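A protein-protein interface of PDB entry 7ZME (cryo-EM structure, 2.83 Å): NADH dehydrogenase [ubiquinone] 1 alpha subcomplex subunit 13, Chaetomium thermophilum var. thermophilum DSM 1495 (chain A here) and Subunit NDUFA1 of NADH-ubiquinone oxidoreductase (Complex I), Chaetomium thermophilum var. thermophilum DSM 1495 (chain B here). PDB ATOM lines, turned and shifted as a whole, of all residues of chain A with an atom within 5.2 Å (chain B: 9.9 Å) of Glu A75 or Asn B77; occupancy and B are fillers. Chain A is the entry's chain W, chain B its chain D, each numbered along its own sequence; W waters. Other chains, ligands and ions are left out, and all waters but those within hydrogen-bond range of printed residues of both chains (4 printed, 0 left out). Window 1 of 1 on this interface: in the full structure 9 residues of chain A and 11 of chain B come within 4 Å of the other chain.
Water W4 lies within hydrogen-bond range of the backbone carbonyl oxygen (O) of Asn B77 (2.6 Å), the side-chain carboxylate (OD2) of Asp A78 (2.7 Å), the guanidinium group (NH2) of Arg A82 (2.9 Å) and the indole nitrogen (NE1) of Trp B79 (3.4 Å). Water W3 lies within hydrogen-bond range of ND2 of Asn B77 (2.8 Å), OE1 of Glu A75 (2.8 Å) and OE2 of Glu A74 (3.4 Å). Water W2 bridges O of Glu B74 (2.8 Å) and OD1 of Asp A78 (3.3 Å). Water W1 lies within hydrogen-bond range of the backbone carbonyl oxygen of Pro B78 (3.2 Å), the side-chain amide nitrogen of Asn B77 (3.2 Å), the side-chain carboxylate of Glu A75 (3.3 Å) and the indole nitrogen of Trp B79 (3.4 Å).
Hydrophobic or aromatic side chains of chain B within 4 Å of the printed part of chain A: Phe B73 and Trp B79. Of the 10 printed residues of chain A, 6 touch a printed residue of chain B. Among the printed residues, 11 pairs touch across the chains.
The guanidinium group (NE) of Arg B52 lies within salt-bridge range of the side-chain carboxylate (OE1) of Glu A74 (3.0 Å). The side-chain amide nitrogen (ND2) of Asn B77 lies within hydrogen-bond range of the side-chain carboxylate (OD2) of Asp A78. The backbone carbonyl oxygen (O) of Glu B74 sits close to the side-chain carboxylate (OD1) of Asp A78, at 3.0 Å. The side-chain carboxylate (OE1) of Glu A75 lies within hydrogen-bond range of the side-chain amide nitrogen (ND2) of Asn B77, at 3.1 Å. OE2 of Glu A74 lies within salt-bridge range of NH1 of Arg B55.
Of the printed residues of chain B, Leu A71 touches Gln B49 (3.3 Å) and Arg B52 (3.8 Å). No residue of chain B comes within 4 Å of Gln A72. Of the printed residues of chain B, Glu A75 touches Asn B77 (3.1 Å). No residue of chain B comes within 4 Å of Asp A76. Of the printed residues of chain B, Asp A78 touches Glu B74, Asn B77 and Trp B79. Of the printed residues of chain B, His A79 touches Trp B79 (3.8 Å). Of the printed residues of chain A, Arg B52 touches Leu A71 and Glu A74. Of the printed residues of chain A, Glu B74 touches Asp A78. Of chain A, only Glu A75 and Asp A78 come within 4 Å of Asn B77. Printed residues of chain A within 4 Å of Trp B79: Asp A78 (3.6 Å), His A79 (3.8 Å) and Arg A82 (3.3 Å).
O of Phe B73 lies close to OD1 of Asn B76, at 2.7 Å. NH1 of Arg B55 lies within hydrogen-bond range of OD1 of Asn B77, 3.2 Å away. The side-chain carboxylate (OE2) of Glu A75 sits at hydrogen-bond distance from a ring nitrogen (NE2) of His A79. O of Arg B55 sits at hydrogen-bond distance from ND2 of Asn B76 (2.9 Å). The backbone carbonyl oxygen of Phe B73 is in hydrogen-bond range of the guanidinium group of Arg B55 (2.8 Å).
Leu A71 touches Gln B49. Arg B52 touches Leu A71. Phe B73 touches Glu A74. NE1 of Trp B79 touches OD2 of Asp A78, at 3.6 Å. CZ2 of Trp B79 touches CE1 of His A79 (3.8 Å). Arg A82 touches Trp B79.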
ATOM      1  N   LEU A  71      -1.099  -1.206  -0.833  1.00  0.00           N
ATOM      2  CA  LEU A  71      -0.365  -0.013  -1.324  1.00  0.00           C
ATOM      3  C   LEU A  71      -0.155  -0.125  -2.834  1.00  0.00           C
ATOM      4  O   LEU A  71      -0.423   0.855  -3.527  1.00  0.00           O
ATOM      5  CB  LEU A  71       0.935   0.138  -0.532  1.00  0.00           C
ATOM      6  CG  LEU A  71       0.779   0.612   0.910  1.00  0.00           C
ATOM      7  CD1 LEU A  71       2.042   0.331   1.704  1.00  0.00           C
ATOM      8  CD2 LEU A  71       0.430   2.086   0.963  1.00  0.00           C
ATOM      9  N   GLN A  72       0.339  -1.264  -3.309  1.00  0.00           N
ATOM     10  CA  GLN A  72       0.583  -1.498  -4.755  1.00  0.00           C
ATOM     11  C   GLN A  72      -0.734  -1.439  -5.526  1.00  0.00           C
ATOM     12  O   GLN A  72      -0.705  -1.008  -6.677  1.00  0.00           O
ATOM     13  CB  GLN A  72       1.328  -2.817  -4.956  1.00  0.00           C
ATOM     14  CG  GLN A  72       1.844  -3.031  -6.370  1.00  0.00           C
ATOM     15  CD  GLN A  72       2.820  -1.976  -6.829  1.00  0.00           C
ATOM     16  OE1 GLN A  72       3.537  -1.373  -6.038  1.00  0.00           O
ATOM     17  NE2 GLN A  72       2.864  -1.758  -8.132  1.00  0.00           N
ATOM     18  N   ALA A  73      -1.850  -1.814  -4.907  1.00  0.00           N
ATOM     19  CA  ALA A  73      -3.153  -1.834  -5.608  1.00  0.00           C
ATOM     20  C   ALA A  73      -3.596  -0.394  -5.869  1.00  0.00           C
ATOM     21  O   ALA A  73      -4.054  -0.125  -6.983  1.00  0.00           O
ATOM     22  CB  ALA A  73      -4.152  -2.543  -4.741  1.00  0.00           C
ATOM     23  N   GLU A  74      -3.433   0.494  -4.893  1.00  0.00           N
ATOM     24  CA  GLU A  74      -3.732   1.932  -5.054  1.00  0.00           C
ATOM     25  C   GLU A  74      -2.810   2.535  -6.104  1.00  0.00           C
ATOM     26  O   GLU A  74      -3.283   3.387  -6.870  1.00  0.00           O
ATOM     27  CB  GLU A  74      -3.424   2.602  -3.725  1.00  0.00           C
ATOM     28  CG  GLU A  74      -3.670   4.097  -3.710  1.00  0.00           C
ATOM     29  CD  GLU A  74      -2.860   4.827  -2.657  1.00  0.00           C
ATOM     30  OE1 GLU A  74      -2.377   4.168  -1.720  1.00  0.00           O
ATOM     31  OE2 GLU A  74      -2.699   6.049  -2.791  1.00  0.00           O
ATOM     32  N   GLU A  75      -1.531   2.150  -6.101  1.00  0.00           N
ATOM     33  CA  GLU A  75      -0.535   2.665  -7.077  1.00  0.00           C
ATOM     34  C   GLU A  75      -0.903   2.220  -8.492  1.00  0.00           C
ATOM     35  O   GLU A  75      -0.772   3.025  -9.414  1.00  0.00           O
ATOM     36  CB  GLU A  75       0.876   2.244  -6.664  1.00  0.00           C
ATOM     37  CG  GLU A  75       1.972   2.882  -7.495  1.00  0.00           C
ATOM     38  CD  GLU A  75       2.139   4.386  -7.348  1.00  0.00           C
ATOM     39  OE1 GLU A  75       1.655   4.945  -6.347  1.00  0.00           O
ATOM     40  OE2 GLU A  75       2.764   4.995  -8.233  1.00  0.00           O
ATOM     41  N   ASP A  76      -1.358   0.981  -8.640  1.00  0.00           N
ATOM     42  CA  ASP A  76      -1.725   0.434  -9.970  1.00  0.00           C
ATOM     43  C   ASP A  76      -2.978   1.127 -10.487  1.00  0.00           C
ATOM     44  O   ASP A  76      -3.039   1.374 -11.689  1.00  0.00           O
ATOM     45  CB  ASP A  76      -2.010  -1.062  -9.901  1.00  0.00           C
ATOM     46  CG  ASP A  76      -0.778  -1.924  -9.732  1.00  0.00           C
ATOM     47  OD1 ASP A  76       0.296  -1.373  -9.437  1.00  0.00           O
ATOM     48  OD2 ASP A  76      -0.910  -3.140  -9.911  1.00  0.00           O
ATOM     49  N   ARG A  77      -3.932   1.419  -9.603  1.00  0.00           N
ATOM     50  CA  ARG A  77      -5.158   2.135 -10.032  1.00  0.00           C
ATOM     51  C   ARG A  77      -4.766   3.510 -10.569  1.00  0.00           C
ATOM     52  O   ARG A  77      -5.361   3.925 -11.564  1.00  0.00           O
ATOM     53  CB  ARG A  77      -6.172   2.197  -8.887  1.00  0.00           C
ATOM     54  CG  ARG A  77      -6.972   0.921  -8.689  1.00  0.00           C
ATOM     55  CD  ARG A  77      -8.058   1.153  -7.663  1.00  0.00           C
ATOM     56  NE  ARG A  77      -7.543   1.316  -6.315  1.00  0.00           N
ATOM     57  CZ  ARG A  77      -7.471   0.342  -5.418  1.00  0.00           C
ATOM     58  NH1 ARG A  77      -7.888  -0.872  -5.726  1.00  0.00           N
ATOM     59  NH2 ARG A  77      -6.987   0.589  -4.216  1.00  0.00           N
ATOM     60  N   ASP A  78      -3.802   4.170  -9.933  1.00  0.00           N
ATOM     61  CA  ASP A  78      -3.304   5.494 -10.385  1.00  0.00           C
ATOM     62  C   ASP A  78      -2.603   5.356 -11.740  1.00  0.00           C
ATOM     63  O   ASP A  78      -2.775   6.247 -12.569  1.00  0.00           O
ATOM     64  CB  ASP A  78      -2.342   6.066  -9.342  1.00  0.00           C
ATOM     65  CG  ASP A  78      -2.122   7.563  -9.468  1.00  0.00           C
ATOM     66  OD1 ASP A  78      -2.920   8.320  -8.888  1.00  0.00           O
ATOM     67  OD2 ASP A  78      -1.149   7.961 -10.138  1.00  0.00           O
ATOM     68  N   HIS A  79      -1.840   4.285 -11.937  1.00  0.00           N
ATOM     69  CA  HIS A  79      -1.088   4.081 -13.194  1.00  0.00           C
ATOM     70  C   HIS A  79      -2.039   3.806 -14.345  1.00  0.00           C
ATOM     71  O   HIS A  79      -1.799   4.365 -15.418  1.00  0.00           O
ATOM     72  CB  HIS A  79      -0.060   2.959 -13.004  1.00  0.00           C
ATOM     73  CG  HIS A  79       1.223   3.443 -12.423  1.00  0.00           C
ATOM     74  ND1 HIS A  79       2.364   3.582 -13.177  1.00  0.00           N
ATOM     75  CD2 HIS A  79       1.538   3.852 -11.177  1.00  0.00           C
ATOM     76  CE1 HIS A  79       3.334   4.032 -12.416  1.00  0.00           C
ATOM     77  NE2 HIS A  79       2.853   4.206 -11.186  1.00  0.00           N
ATOM     78  N   ARG A  82      -3.823   7.142 -15.171  1.00  0.00           N
ATOM     79  CA  ARG A  82      -2.944   8.095 -15.901  1.00  0.00           C
ATOM     80  C   ARG A  82      -2.625   7.587 -17.302  1.00  0.00           C
ATOM     81  O   ARG A  82      -2.485   8.426 -18.198  1.00  0.00           O
ATOM     82  CB  ARG A  82      -1.738   8.532 -15.064  1.00  0.00           C
ATOM     83  CG  ARG A  82      -2.130   9.247 -13.782  1.00  0.00           C
ATOM     84  CD  ARG A  82      -0.995  10.006 -13.134  1.00  0.00           C
ATOM     85  NE  ARG A  82      -0.531  11.108 -13.955  1.00  0.00           N
ATOM     86  CZ  ARG A  82       0.240  12.093 -13.519  1.00  0.00           C
ATOM     87  NH1 ARG A  82       0.613  13.054 -14.343  1.00  0.00           N
ATOM     88  NH2 ARG A  82       0.624  12.123 -12.258  1.00  0.00           N
ATOM     89  N   GLN B  44      13.691   4.021   0.868  1.00  0.00           N
ATOM     90  CA  GLN B  44      12.666   4.363  -0.143  1.00  0.00           C
ATOM     91  C   GLN B  44      11.256   4.157   0.413  1.00  0.00           C
ATOM     92  O   GLN B  44      10.405   5.003   0.133  1.00  0.00           O
ATOM     93  CB  GLN B  44      12.934   3.618  -1.452  1.00  0.00           C
ATOM     94  CG  GLN B  44      12.007   4.002  -2.599  1.00  0.00           C
ATOM     95  CD  GLN B  44      11.951   5.477  -2.932  1.00  0.00           C
ATOM     96  OE1 GLN B  44      10.973   5.963  -3.490  1.00  0.00           O
ATOM     97  NE2 GLN B  44      13.004   6.210  -2.606  1.00  0.00           N
ATOM     98  N   LYS B  47      10.290   7.003   2.747  1.00  0.00           N
ATOM     99  CA  LYS B  47      10.181   8.300   2.049  1.00  0.00           C
ATOM    100  C   LYS B  47       8.887   8.262   1.253  1.00  0.00           C
ATOM    101  O   LYS B  47       8.217   9.301   1.207  1.00  0.00           O
ATOM    102  CB  LYS B  47      11.370   8.433   1.096  1.00  0.00           C
ATOM    103  CG  LYS B  47      12.726   8.686   1.733  1.00  0.00           C
ATOM    104  CD  LYS B  47      13.842   8.699   0.710  1.00  0.00           C
ATOM    105  CE  LYS B  47      15.208   8.955   1.307  1.00  0.00           C
ATOM    106  NZ  LYS B  47      15.648   7.839   2.177  1.00  0.00           N
ATOM    107  N   GLN B  48       8.544   7.107   0.685  1.00  0.00           N
ATOM    108  CA  GLN B  48       7.245   6.918  -0.006  1.00  0.00           C
ATOM    109  C   GLN B  48       6.083   6.989   0.982  1.00  0.00           C
ATOM    110  O   GLN B  48       5.013   7.428   0.565  1.00  0.00           O
ATOM    111  CB  GLN B  48       7.269   5.584  -0.747  1.00  0.00           C
ATOM    112  CG  GLN B  48       8.092   5.567  -2.018  1.00  0.00           C
ATOM    113  CD  GLN B  48       7.920   4.234  -2.699  1.00  0.00           C
ATOM    114  OE1 GLN B  48       7.076   3.434  -2.316  1.00  0.00           O
ATOM    115  NE2 GLN B  48       8.712   3.991  -3.727  1.00  0.00           N
ATOM    116  N   GLN B  49       6.285   6.573   2.229  1.00  0.00           N
ATOM    117  CA  GLN B  49       5.210   6.570   3.258  1.00  0.00           C
ATOM    118  C   GLN B  49       4.990   7.991   3.781  1.00  0.00           C
ATOM    119  O   GLN B  49       3.847   8.320   4.092  1.00  0.00           O
ATOM    120  CB  GLN B  49       5.533   5.563   4.358  1.00  0.00           C
ATOM    121  CG  GLN B  49       5.311   4.111   3.964  1.00  0.00           C
ATOM    122  CD  GLN B  49       3.866   3.678   3.921  1.00  0.00           C
ATOM    123  OE1 GLN B  49       2.944   4.451   4.160  1.00  0.00           O
ATOM    124  NE2 GLN B  49       3.656   2.410   3.618  1.00  0.00           N
ATOM    125  N   MET B  50       6.057   8.782   3.904  1.00  0.00           N
ATOM    126  CA  MET B  50       5.949  10.198   4.335  1.00  0.00           C
ATOM    127  C   MET B  50       5.248  11.009   3.249  1.00  0.00           C
ATOM    128  O   MET B  50       4.502  11.930   3.599  1.00  0.00           O
ATOM    129  CB  MET B  50       7.314  10.792   4.691  1.00  0.00           C
ATOM    130  CG  MET B  50       7.778  10.370   6.070  1.00  0.00           C
ATOM    131  SD  MET B  50       9.398  10.992   6.566  1.00  0.00           S
ATOM    132  CE  MET B  50      10.448  10.224   5.335  1.00  0.00           C
ATOM    133  N   GLU B  51       5.455  10.647   1.983  1.00  0.00           N
ATOM    134  CA  GLU B  51       4.869  11.419   0.865  1.00  0.00           C
ATOM    135  C   GLU B  51       3.402  11.022   0.776  1.00  0.00           C
ATOM    136  O   GLU B  51       2.595  11.875   0.383  1.00  0.00           O
ATOM    137  CB  GLU B  51       5.613  11.084  -0.421  1.00  0.00           C
ATOM    138  CG  GLU B  51       6.895  11.871  -0.597  1.00  0.00           C
ATOM    139  CD  GLU B  51       7.833  11.281  -1.634  1.00  0.00           C
ATOM    140  OE1 GLU B  51       7.637  10.104  -1.997  1.00  0.00           O
ATOM    141  OE2 GLU B  51       8.753  11.999  -2.075  1.00  0.00           O
ATOM    142  N   ARG B  52       3.078   9.786   1.148  1.00  0.00           N
ATOM    143  CA  ARG B  52       1.657   9.366   1.218  1.00  0.00           C
ATOM    144  C   ARG B  52       0.955  10.110   2.361  1.00  0.00           C
ATOM    145  O   ARG B  52      -0.228  10.412   2.216  1.00  0.00           O
ATOM    146  CB  ARG B  52       1.538   7.840   1.213  1.00  0.00           C
ATOM    147  CG  ARG B  52       0.120   7.351   0.962  1.00  0.00           C
ATOM    148  CD  ARG B  52      -0.035   5.851   0.834  1.00  0.00           C
ATOM    149  NE  ARG B  52      -1.448   5.505   0.852  1.00  0.00           N
ATOM    150  CZ  ARG B  52      -2.115   5.140   1.938  1.00  0.00           C
ATOM    151  NH1 ARG B  52      -1.492   5.045   3.098  1.00  0.00           N
ATOM    152  NH2 ARG B  52      -3.401   4.858   1.859  1.00  0.00           N
ATOM    153  N   ASP B  53       1.642  10.350   3.471  1.00  0.00           N
ATOM    154  CA  ASP B  53       1.075  11.103   4.627  1.00  0.00           C
ATOM    155  C   ASP B  53       0.753  12.554   4.244  1.00  0.00           C
ATOM    156  O   ASP B  53      -0.272  13.057   4.705  1.00  0.00           O
ATOM    157  CB  ASP B  53       2.029  11.069   5.823  1.00  0.00           C
ATOM    158  CG  ASP B  53       2.135   9.715   6.493  1.00  0.00           C
ATOM    159  OD1 ASP B  53       1.367   8.818   6.121  1.00  0.00           O
ATOM    160  OD2 ASP B  53       2.990   9.576   7.382  1.00  0.00           O
ATOM    161  N   ARG B  54       1.615  13.210   3.466  1.00  0.00           N
ATOM    162  CA  ARG B  54       1.359  14.589   2.975  1.00  0.00           C
ATOM    163  C   ARG B  54       0.117  14.549   2.085  1.00  0.00           C
ATOM    164  O   ARG B  54      -0.658  15.506   2.115  1.00  0.00           O
ATOM    165  CB  ARG B  54       2.598  15.136   2.263  1.00  0.00           C
ATOM    166  CG  ARG B  54       2.556  16.631   1.991  1.00  0.00           C
ATOM    167  CD  ARG B  54       3.242  17.066   0.714  1.00  0.00           C
ATOM    168  NE  ARG B  54       4.644  17.432   0.854  1.00  0.00           N
ATOM    169  CZ  ARG B  54       5.645  16.805   0.254  1.00  0.00           C
ATOM    170  NH1 ARG B  54       6.887  17.223   0.431  1.00  0.00           N
ATOM    171  NH2 ARG B  54       5.402  15.769  -0.526  1.00  0.00           N
ATOM    172  N   ARG B  55      -0.066  13.468   1.330  1.00  0.00           N
ATOM    173  CA  ARG B  55      -1.259  13.300   0.469  1.00  0.00           C
ATOM    174  C   ARG B  55      -2.541  13.310   1.312  1.00  0.00           C
ATOM    175  O   ARG B  55      -3.560  13.792   0.799  1.00  0.00           O
ATOM    176  CB  ARG B  55      -1.126  12.034  -0.376  1.00  0.00           C
ATOM    177  CG  ARG B  55      -0.129  12.126  -1.518  1.00  0.00           C
ATOM    178  CD  ARG B  55      -0.050  10.774  -2.193  1.00  0.00           C
ATOM    179  NE  ARG B  55      -1.316  10.405  -2.804  1.00  0.00           N
ATOM    180  CZ  ARG B  55      -1.623   9.180  -3.205  1.00  0.00           C
ATOM    181  NH1 ARG B  55      -0.757   8.196  -3.042  1.00  0.00           N
ATOM    182  NH2 ARG B  55      -2.797   8.941  -3.759  1.00  0.00           N
ATOM    183  N   LEU B  56      -2.515  12.765   2.530  1.00  0.00           N
ATOM    184  CA  LEU B  56      -3.740  12.683   3.369  1.00  0.00           C
ATOM    185  C   LEU B  56      -3.835  13.858   4.353  1.00  0.00           C
ATOM    186  O   LEU B  56      -4.963  14.259   4.644  1.00  0.00           O
ATOM    187  CB  LEU B  56      -3.706  11.355   4.130  1.00  0.00           C
ATOM    188  CG  LEU B  56      -3.852  10.083   3.298  1.00  0.00           C
ATOM    189  CD1 LEU B  56      -3.005   8.958   3.868  1.00  0.00           C
ATOM    190  CD2 LEU B  56      -5.308   9.660   3.210  1.00  0.00           C
ATOM    191  N   GLY B  72     -10.425  13.350  -3.649  1.00  0.00           N
ATOM    192  CA  GLY B  72      -9.274  13.972  -4.333  1.00  0.00           C
ATOM    193  C   GLY B  72      -7.983  13.243  -4.042  1.00  0.00           C
ATOM    194  O   GLY B  72      -6.981  13.621  -4.642  1.00  0.00           O
ATOM    195  N   PHE B  73      -8.009  12.234  -3.163  1.00  0.00           N
ATOM    196  CA  PHE B  73      -6.812  11.425  -2.807  1.00  0.00           C
ATOM    197  C   PHE B  73      -6.350  10.653  -4.040  1.00  0.00           C
ATOM    198  O   PHE B  73      -5.145  10.473  -4.219  1.00  0.00           O
ATOM    199  CB  PHE B  73      -7.068  10.540  -1.590  1.00  0.00           C
ATOM    200  CG  PHE B  73      -5.886   9.725  -1.140  1.00  0.00           C
ATOM    201  CD1 PHE B  73      -4.815  10.323  -0.498  1.00  0.00           C
ATOM    202  CD2 PHE B  73      -5.846   8.358  -1.355  1.00  0.00           C
ATOM    203  CE1 PHE B  73      -3.726   9.571  -0.088  1.00  0.00           C
ATOM    204  CE2 PHE B  73      -4.758   7.610  -0.939  1.00  0.00           C
ATOM    205  CZ  PHE B  73      -3.702   8.218  -0.307  1.00  0.00           C
ATOM    206  N   GLU B  74      -7.118  10.203  -4.884  1.00  0.00           N
ATOM    207  CA  GLU B  74      -6.749   9.367  -6.050  1.00  0.00           C
ATOM    208  C   GLU B  74      -6.144  10.222  -7.167  1.00  0.00           C
ATOM    209  O   GLU B  74      -5.516   9.653  -8.053  1.00  0.00           O
ATOM    210  CB  GLU B  74      -8.083   8.791  -6.504  1.00  0.00           C
ATOM    211  CG  GLU B  74      -9.242   9.645  -6.031  1.00  0.00           C
ATOM    212  CD  GLU B  74     -10.560   9.432  -6.747  1.00  0.00           C
ATOM    213  OE1 GLU B  74     -11.597   9.838  -6.194  1.00  0.00           O
ATOM    214  OE2 GLU B  74     -10.544   8.875  -7.861  1.00  0.00           O
ATOM    215  N   PHE B  75      -6.448  11.576  -7.137  1.00  0.00           N
ATOM    216  CA  PHE B  75      -5.823  12.513  -8.100  1.00  0.00           C
ATOM    217  C   PHE B  75      -4.616  13.244  -7.505  1.00  0.00           C
ATOM    218  O   PHE B  75      -3.950  13.941  -8.277  1.00  0.00           O
ATOM    219  CB  PHE B  75      -6.852  13.573  -8.484  1.00  0.00           C
ATOM    220  CG  PHE B  75      -8.205  13.043  -8.878  1.00  0.00           C
ATOM    221  CD1 PHE B  75      -8.431  12.558 -10.153  1.00  0.00           C
ATOM    222  CD2 PHE B  75      -9.257  13.047  -7.977  1.00  0.00           C
ATOM    223  CE1 PHE B  75      -9.678  12.082 -10.517  1.00  0.00           C
ATOM    224  CE2 PHE B  75     -10.506  12.578  -8.347  1.00  0.00           C
ATOM    225  CZ  PHE B  75     -10.713  12.093  -9.615  1.00  0.00           C
ATOM    226  N   ASN B  76      -4.309  13.077  -6.214  1.00  0.00           N
ATOM    227  CA  ASN B  76      -3.221  13.878  -5.576  1.00  0.00           C
ATOM    228  C   ASN B  76      -1.897  13.116  -5.554  1.00  0.00           C
ATOM    229  O   ASN B  76      -0.991  13.568  -4.852  1.00  0.00           O
ATOM    230  CB  ASN B  76      -3.608  14.467  -4.209  1.00  0.00           C
ATOM    231  CG  ASN B  76      -3.777  13.472  -3.081  1.00  0.00           C
ATOM    232  OD1 ASN B  76      -3.423  12.306  -3.197  1.00  0.00           O
ATOM    233  ND2 ASN B  76      -4.303  13.938  -1.963  1.00  0.00           N
ATOM    234  N   ASN B  77      -1.787  12.026  -6.312  1.00  0.00           N
ATOM    235  CA  ASN B  77      -0.560  11.192  -6.235  1.00  0.00           C
ATOM    236  C   ASN B  77       0.535  11.934  -7.001  1.00  0.00           C
ATOM    237  O   ASN B  77       0.347  12.194  -8.196  1.00  0.00           O
ATOM    238  CB  ASN B  77      -0.758   9.771  -6.755  1.00  0.00           C
ATOM    239  CG  ASN B  77       0.373   8.832  -6.398  1.00  0.00           C
ATOM    240  OD1 ASN B  77       1.159   9.107  -5.498  1.00  0.00           O
ATOM    241  ND2 ASN B  77       0.451   7.709  -7.089  1.00  0.00           N
ATOM    242  N   PRO B  78       1.639  12.377  -6.356  1.00  0.00           N
ATOM    243  CA  PRO B  78       2.653  13.186  -7.037  1.00  0.00           C
ATOM    244  C   PRO B  78       3.520  12.317  -7.932  1.00  0.00           C
ATOM    245  O   PRO B  78       4.000  11.261  -7.518  1.00  0.00           O
ATOM    246  CB  PRO B  78       3.466  13.787  -5.882  1.00  0.00           C
ATOM    247  CG  PRO B  78       2.727  13.411  -4.624  1.00  0.00           C
ATOM    248  CD  PRO B  78       1.996  12.156  -4.950  1.00  0.00           C
ATOM    249  N   TRP B  79       3.710  12.761  -9.165  1.00  0.00           N
ATOM    250  CA  TRP B  79       4.664  12.148 -10.073  1.00  0.00           C
ATOM    251  C   TRP B  79       5.822  13.119 -10.251  1.00  0.00           C
ATOM    252  O   TRP B  79       5.628  14.237 -10.734  1.00  0.00           O
ATOM    253  CB  TRP B  79       4.008  11.799 -11.407  1.00  0.00           C
ATOM    254  CG  TRP B  79       3.320  10.475 -11.374  1.00  0.00           C
ATOM    255  CD1 TRP B  79       2.942   9.786 -10.268  1.00  0.00           C
ATOM    256  CD2 TRP B  79       2.932   9.677 -12.496  1.00  0.00           C
ATOM    257  NE1 TRP B  79       2.341   8.609 -10.622  1.00  0.00           N
ATOM    258  CE2 TRP B  79       2.320   8.518 -11.988  1.00  0.00           C
ATOM    259  CE3 TRP B  79       3.041   9.832 -13.882  1.00  0.00           C
ATOM    260  CZ2 TRP B  79       1.820   7.518 -12.812  1.00  0.00           C
ATOM    261  CZ3 TRP B  79       2.544   8.837 -14.699  1.00  0.00           C
ATOM    262  CH2 TRP B  79       1.942   7.695 -14.160  1.00  0.00           C
ATOM    263  N   LYS B  80       7.015  12.692  -9.849  1.00  0.00           N
ATOM    264  CA  LYS B  80       8.156  13.591  -9.812  1.00  0.00           C
ATOM    265  C   LYS B  80       8.596  13.948 -11.224  1.00  0.00           C
ATOM    266  O   LYS B  80       8.691  13.087 -12.100  1.00  0.00           O
ATOM    267  CB  LYS B  80       9.316  12.948  -9.057  1.00  0.00           C
ATOM    268  CG  LYS B  80       9.000  12.526  -7.641  1.00  0.00           C
ATOM    269  CD  LYS B  80       8.515  13.667  -6.795  1.00  0.00           C
ATOM    270  CE  LYS B  80       8.035  13.151  -5.456  1.00  0.00           C
ATOM    271  NZ  LYS B  80       6.557  13.191  -5.347  1.00  0.00           N
ATOM    272  N   VAL B  81       8.882  15.226 -11.441  1.00  0.00           N
ATOM    273  CA  VAL B  81       9.254  15.739 -12.752  1.00  0.00           C
ATOM    274  C   VAL B  81      10.678  16.267 -12.661  1.00  0.00           C
ATOM    275  O   VAL B  81      10.972  17.140 -11.836  1.00  0.00           O
ATOM    276  CB  VAL B  81       8.290  16.835 -13.225  1.00  0.00           C
ATOM    277  CG1 VAL B  81       8.606  17.232 -14.638  1.00  0.00           C
ATOM    278  CG2 VAL B  81       6.859  16.362 -13.114  1.00  0.00           C
HETATM  279  O   HOH W   1       3.638   8.056  -7.577  1.00  0.00           O
HETATM  280  O   HOH W   2      -5.969   7.007  -8.948  1.00  0.00           O
HETATM  281  O   HOH W   3      -0.955   5.743  -5.674  1.00  0.00           O
HETATM  282  O   HOH W   4      -0.416  10.537 -10.076  1.00  0.00           O
